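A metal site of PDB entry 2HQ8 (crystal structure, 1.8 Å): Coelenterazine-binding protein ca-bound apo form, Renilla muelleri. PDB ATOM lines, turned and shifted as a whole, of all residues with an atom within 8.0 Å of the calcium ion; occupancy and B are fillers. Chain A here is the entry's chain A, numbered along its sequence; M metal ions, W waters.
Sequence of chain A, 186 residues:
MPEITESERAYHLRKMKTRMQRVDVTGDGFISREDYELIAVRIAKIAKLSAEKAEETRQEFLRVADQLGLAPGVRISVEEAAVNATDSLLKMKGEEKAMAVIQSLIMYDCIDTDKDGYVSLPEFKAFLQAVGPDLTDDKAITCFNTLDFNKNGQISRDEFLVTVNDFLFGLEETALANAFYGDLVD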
ATOM      1  N   TYR A 118      -7.166  17.772  32.702  1.00  0.00           N
ATOM      2  CA  TYR A 118      -6.255  17.253  31.673  1.00  0.00           C
ATOM      3  C   TYR A 118      -5.054  16.628  32.377  1.00  0.00           C
ATOM      4  O   TYR A 118      -4.696  17.035  33.477  1.00  0.00           O
ATOM      5  CB  TYR A 118      -5.739  18.382  30.786  1.00  0.00           C
ATOM      6  CG  TYR A 118      -6.867  19.011  30.005  1.00  0.00           C
ATOM      7  CD1 TYR A 118      -7.432  18.338  28.914  1.00  0.00           C
ATOM      8  CD2 TYR A 118      -7.384  20.238  30.384  1.00  0.00           C
ATOM      9  CE1 TYR A 118      -8.496  18.906  28.200  1.00  0.00           C
ATOM     10  CE2 TYR A 118      -8.429  20.819  29.668  1.00  0.00           C
ATOM     11  CZ  TYR A 118      -8.972  20.141  28.601  1.00  0.00           C
ATOM     12  OH  TYR A 118     -10.014  20.728  27.910  1.00  0.00           O
ATOM     13  N   VAL A 119      -4.438  15.667  31.703  1.00  0.00           N
ATOM     14  CA  VAL A 119      -3.176  15.085  32.190  1.00  0.00           C
ATOM     15  C   VAL A 119      -2.017  15.676  31.389  1.00  0.00           C
ATOM     16  O   VAL A 119      -1.905  15.451  30.174  1.00  0.00           O
ATOM     17  CB  VAL A 119      -3.200  13.530  32.154  1.00  0.00           C
ATOM     18  CG1 VAL A 119      -1.783  12.942  32.299  1.00  0.00           C
ATOM     19  CG2 VAL A 119      -4.112  13.020  33.234  1.00  0.00           C
ATOM     20  N   PHE A 144       4.220   9.425  26.885  1.00  0.00           N
ATOM     21  CA  PHE A 144       3.289  10.529  26.848  1.00  0.00           C
ATOM     22  C   PHE A 144       2.899  10.851  25.402  1.00  0.00           C
ATOM     23  O   PHE A 144       1.709  11.009  25.098  1.00  0.00           O
ATOM     24  CB  PHE A 144       3.928  11.774  27.504  1.00  0.00           C
ATOM     25  CG  PHE A 144       3.061  12.999  27.421  1.00  0.00           C
ATOM     26  CD1 PHE A 144       2.071  13.235  28.388  1.00  0.00           C
ATOM     27  CD2 PHE A 144       3.249  13.923  26.394  1.00  0.00           C
ATOM     28  CE1 PHE A 144       1.272  14.357  28.325  1.00  0.00           C
ATOM     29  CE2 PHE A 144       2.438  15.067  26.309  1.00  0.00           C
ATOM     30  CZ  PHE A 144       1.440  15.283  27.282  1.00  0.00           C
ATOM     31  N   ASN A 145       3.889  10.921  24.509  1.00  0.00           N
ATOM     32  CA  ASN A 145       3.574  11.284  23.120  1.00  0.00           C
ATOM     33  C   ASN A 145       2.657  10.238  22.470  1.00  0.00           C
ATOM     34  O   ASN A 145       1.815  10.576  21.625  1.00  0.00           O
ATOM     35  CB  ASN A 145       4.845  11.480  22.310  1.00  0.00           C
ATOM     36  CG  ASN A 145       5.613  12.717  22.743  1.00  0.00           C
ATOM     37  OD1 ASN A 145       5.042  13.642  23.323  1.00  0.00           O
ATOM     38  ND2 ASN A 145       6.892  12.738  22.436  1.00  0.00           N
ATOM     39  N   LEU A 147       0.190   8.488  24.000  1.00  0.00           N
ATOM     40  CA  LEU A 147      -1.171   8.789  24.447  1.00  0.00           C
ATOM     41  C   LEU A 147      -1.713  10.115  23.881  1.00  0.00           C
ATOM     42  O   LEU A 147      -2.920  10.301  23.780  1.00  0.00           O
ATOM     43  CB  LEU A 147      -1.224   8.803  25.968  1.00  0.00           C
ATOM     44  CG  LEU A 147      -1.557   7.393  26.507  1.00  0.00           C
ATOM     45  CD1 LEU A 147      -0.402   6.458  26.252  1.00  0.00           C
ATOM     46  CD2 LEU A 147      -1.953   7.388  27.958  1.00  0.00           C
ATOM     47  N   ASP A 148      -0.814  11.039  23.538  1.00  0.00           N
ATOM     48  CA  ASP A 148      -1.199  12.353  23.049  1.00  0.00           C
ATOM     49  C   ASP A 148      -1.481  12.280  21.540  1.00  0.00           C
ATOM     50  O   ASP A 148      -0.659  12.724  20.712  1.00  0.00           O
ATOM     51  CB  ASP A 148      -0.084  13.369  23.344  1.00  0.00           C
ATOM     52  CG  ASP A 148      -0.456  14.789  22.965  1.00  0.00           C
ATOM     53  OD1 ASP A 148      -1.654  15.056  22.680  1.00  0.00           O
ATOM     54  OD2 ASP A 148       0.456  15.632  22.946  1.00  0.00           O
ATOM     55  N   PHE A 149      -2.621  11.661  21.203  1.00  0.00           N
ATOM     56  CA  PHE A 149      -3.001  11.346  19.820  1.00  0.00           C
ATOM     57  C   PHE A 149      -2.938  12.582  18.932  1.00  0.00           C
ATOM     58  O   PHE A 149      -2.438  12.501  17.794  1.00  0.00           O
ATOM     59  CB  PHE A 149      -4.428  10.773  19.772  1.00  0.00           C
ATOM     60  CG  PHE A 149      -4.520   9.298  20.098  1.00  0.00           C
ATOM     61  CD1 PHE A 149      -4.246   8.834  21.388  1.00  0.00           C
ATOM     62  CD2 PHE A 149      -4.911   8.376  19.117  1.00  0.00           C
ATOM     63  CE1 PHE A 149      -4.330   7.486  21.699  1.00  0.00           C
ATOM     64  CE2 PHE A 149      -5.021   7.009  19.419  1.00  0.00           C
ATOM     65  CZ  PHE A 149      -4.734   6.569  20.735  1.00  0.00           C
ATOM     66  N   ASN A 150      -3.452  13.708  19.420  1.00  0.00           N
ATOM     67  CA  ASN A 150      -3.472  14.924  18.608  1.00  0.00           C
ATOM     68  C   ASN A 150      -2.252  15.818  18.748  1.00  0.00           C
ATOM     69  O   ASN A 150      -2.217  16.925  18.202  1.00  0.00           O
ATOM     70  CB  ASN A 150      -4.789  15.731  18.795  1.00  0.00           C
ATOM     71  CG  ASN A 150      -4.995  16.263  20.216  1.00  0.00           C
ATOM     72  OD1 ASN A 150      -4.156  16.107  21.114  1.00  0.00           O
ATOM     73  ND2 ASN A 150      -6.141  16.906  20.422  1.00  0.00           N
ATOM     74  N   LYS A 151      -1.276  15.352  19.526  1.00  0.00           N
ATOM     75  CA  LYS A 151      -0.006  16.065  19.731  1.00  0.00           C
ATOM     76  C   LYS A 151      -0.210  17.513  20.205  1.00  0.00           C
ATOM     77  O   LYS A 151       0.566  18.404  19.871  1.00  0.00           O
ATOM     78  CB  LYS A 151       0.877  15.962  18.469  1.00  0.00           C
ATOM     79  CG  LYS A 151       1.343  14.533  18.147  1.00  0.00           C
ATOM     80  CD  LYS A 151       2.137  13.928  19.315  1.00  0.00           C
ATOM     81  CE  LYS A 151       2.586  12.491  19.040  1.00  0.00           C
ATOM     82  NZ  LYS A 151       1.512  11.455  18.869  1.00  0.00           N
ATOM     83  N   ASN A 152      -1.214  17.753  21.045  1.00  0.00           N
ATOM     84  CA  ASN A 152      -1.449  19.124  21.536  1.00  0.00           C
ATOM     85  C   ASN A 152      -0.735  19.411  22.876  1.00  0.00           C
ATOM     86  O   ASN A 152      -0.916  20.463  23.482  1.00  0.00           O
ATOM     87  CB  ASN A 152      -2.956  19.480  21.573  1.00  0.00           C
ATOM     88  CG  ASN A 152      -3.689  18.804  22.735  1.00  0.00           C
ATOM     89  OD1 ASN A 152      -3.185  17.848  23.333  1.00  0.00           O
ATOM     90  ND2 ASN A 152      -4.841  19.324  23.078  1.00  0.00           N
ATOM     91  N   GLY A 153       0.084  18.465  23.328  1.00  0.00           N
ATOM     92  CA  GLY A 153       0.799  18.629  24.624  1.00  0.00           C
ATOM     93  C   GLY A 153       0.034  18.261  25.893  1.00  0.00           C
ATOM     94  O   GLY A 153       0.515  18.511  27.009  1.00  0.00           O
ATOM     95  N   GLN A 154      -1.179  17.726  25.765  1.00  0.00           N
ATOM     96  CA  GLN A 154      -1.892  17.168  26.918  1.00  0.00           C
ATOM     97  C   GLN A 154      -2.609  15.875  26.570  1.00  0.00           C
ATOM     98  O   GLN A 154      -2.989  15.652  25.431  1.00  0.00           O
ATOM     99  CB  GLN A 154      -2.876  18.160  27.592  1.00  0.00           C
ATOM    100  CG  GLN A 154      -3.358  19.267  26.762  1.00  0.00           C
ATOM    101  CD  GLN A 154      -4.357  20.183  27.459  1.00  0.00           C
ATOM    102  OE1 GLN A 154      -4.148  20.675  28.594  1.00  0.00           O
ATOM    103  NE2 GLN A 154      -5.436  20.440  26.764  1.00  0.00           N
ATOM    104  N   ILE A 155      -2.770  15.011  27.565  1.00  0.00           N
ATOM    105  CA  ILE A 155      -3.584  13.799  27.379  1.00  0.00           C
ATOM    106  C   ILE A 155      -4.975  14.166  27.892  1.00  0.00           C
ATOM    107  O   ILE A 155      -5.144  14.503  29.054  1.00  0.00           O
ATOM    108  CB  ILE A 155      -3.017  12.578  28.151  1.00  0.00           C
ATOM    109  CG1 ILE A 155      -1.593  12.213  27.650  1.00  0.00           C
ATOM    110  CG2 ILE A 155      -4.009  11.389  28.054  1.00  0.00           C
ATOM    111  CD1 ILE A 155      -0.791  11.236  28.607  1.00  0.00           C
ATOM    112  N   SER A 156      -5.957  14.183  27.003  1.00  0.00           N
ATOM    113  CA  SER A 156      -7.341  14.419  27.423  1.00  0.00           C
ATOM    114  C   SER A 156      -8.014  13.094  27.817  1.00  0.00           C
ATOM    115  O   SER A 156      -7.511  12.023  27.542  1.00  0.00           O
ATOM    116  CB  SER A 156      -8.118  15.079  26.281  1.00  0.00           C
ATOM    117  OG  SER A 156      -7.874  14.388  25.070  1.00  0.00           O
ATOM    118  N   ARG A 157      -9.188  13.187  28.429  1.00  0.00           N
ATOM    119  CA  ARG A 157      -9.914  12.004  28.867  1.00  0.00           C
ATOM    120  C   ARG A 157     -10.235  11.055  27.709  1.00  0.00           C
ATOM    121  O   ARG A 157     -10.142   9.844  27.887  1.00  0.00           O
ATOM    122  CB  ARG A 157     -11.158  12.431  29.652  1.00  0.00           C
ATOM    123  CG  ARG A 157     -11.674  11.448  30.657  1.00  0.00           C
ATOM    124  CD  ARG A 157     -12.989  12.001  31.276  1.00  0.00           C
ATOM    125  NE  ARG A 157     -12.771  13.300  31.925  1.00  0.00           N
ATOM    126  CZ  ARG A 157     -12.411  13.445  33.199  1.00  0.00           C
ATOM    127  NH1 ARG A 157     -12.234  12.385  33.991  1.00  0.00           N
ATOM    128  NH2 ARG A 157     -12.243  14.680  33.697  1.00  0.00           N
ATOM    129  N   ASP A 158     -10.578  11.567  26.525  1.00  0.00           N
ATOM    130  CA  ASP A 158     -10.836  10.713  25.346  1.00  0.00           C
ATOM    131  C   ASP A 158      -9.615   9.914  24.939  1.00  0.00           C
ATOM    132  O   ASP A 158      -9.714   8.738  24.638  1.00  0.00           O
ATOM    133  CB  ASP A 158     -11.291  11.522  24.126  1.00  0.00           C
ATOM    134  CG  ASP A 158     -10.282  12.578  23.716  1.00  0.00           C
ATOM    135  OD1 ASP A 158     -10.075  13.497  24.513  1.00  0.00           O
ATOM    136  OD2 ASP A 158      -9.724  12.518  22.599  1.00  0.00           O
ATOM    137  N   GLU A 159      -8.448  10.573  24.903  1.00  0.00           N
ATOM    138  CA  GLU A 159      -7.188   9.888  24.600  1.00  0.00           C
ATOM    139  C   GLU A 159      -6.854   8.781  25.623  1.00  0.00           C
ATOM    140  O   GLU A 159      -6.455   7.645  25.260  1.00  0.00           O
ATOM    141  CB  GLU A 159      -6.077  10.955  24.570  1.00  0.00           C
ATOM    142  CG  GLU A 159      -6.247  11.854  23.331  1.00  0.00           C
ATOM    143  CD  GLU A 159      -5.230  12.962  23.247  1.00  0.00           C
ATOM    144  OE1 GLU A 159      -4.695  13.339  24.312  1.00  0.00           O
ATOM    145  OE2 GLU A 159      -4.979  13.454  22.104  1.00  0.00           O
ATOM    146  N   PHE A 160      -6.998   9.122  26.900  1.00  0.00           N
ATOM    147  CA  PHE A 160      -6.804   8.141  27.958  1.00  0.00           C
ATOM    148  C   PHE A 160      -7.755   6.981  27.813  1.00  0.00           C
ATOM    149  O   PHE A 160      -7.337   5.845  27.921  1.00  0.00           O
ATOM    150  CB  PHE A 160      -6.980   8.780  29.329  1.00  0.00           C
ATOM    151  CG  PHE A 160      -6.567   7.889  30.479  1.00  0.00           C
ATOM    152  CD1 PHE A 160      -5.235   7.853  30.889  1.00  0.00           C
ATOM    153  CD2 PHE A 160      -7.531   7.159  31.199  1.00  0.00           C
ATOM    154  CE1 PHE A 160      -4.842   7.073  32.007  1.00  0.00           C
ATOM    155  CE2 PHE A 160      -7.152   6.366  32.305  1.00  0.00           C
ATOM    156  CZ  PHE A 160      -5.806   6.324  32.698  1.00  0.00           C
HETATM  157 CA    CA M   1      -3.886  15.510  23.303  1.00  0.00          CA
HETATM  158  O   HOH W   1      -6.051  16.346  23.860  1.00  0.00           O
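Water W1 lies within hydrogen-bond range of OG of Ser 156, ND2 of Asn 152 and ND2 of Asn 150.
The nearest printed residue that does not touch the calcium ion is Ile 155 (4.4 Å).
The calcium ion is bound by the side-chain amide oxygen (OD1) of Asn 150 (2.3 Å), the backbone carbonyl oxygen (O) of Gln 154 (2.3 Å), the side-chain carboxylate (OD1) of Asp 148 (2.4 Å), water W1 (2.4 Å), the side-chain amide oxygen (OD1) of Asn 152 (2.4 Å), the side-chain carboxylate (OE1) of Glu 159 (2.5 Å) and the side-chain carboxylate (OE2) of Glu 159 (2.6 Å).
O of Asp 148 lies within hydrogen-bond range of NZ of Lys 151, at 3.1 Å.
The side-chain carboxylate of Asp 148 lies within hydrogen-bond range of the backbone NH of Gly 153.
OE1 of Glu 159 sits close to N of Ser 156.
N of Phe 149 sits close to OE2 of Glu 159, 3.1 Å away.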
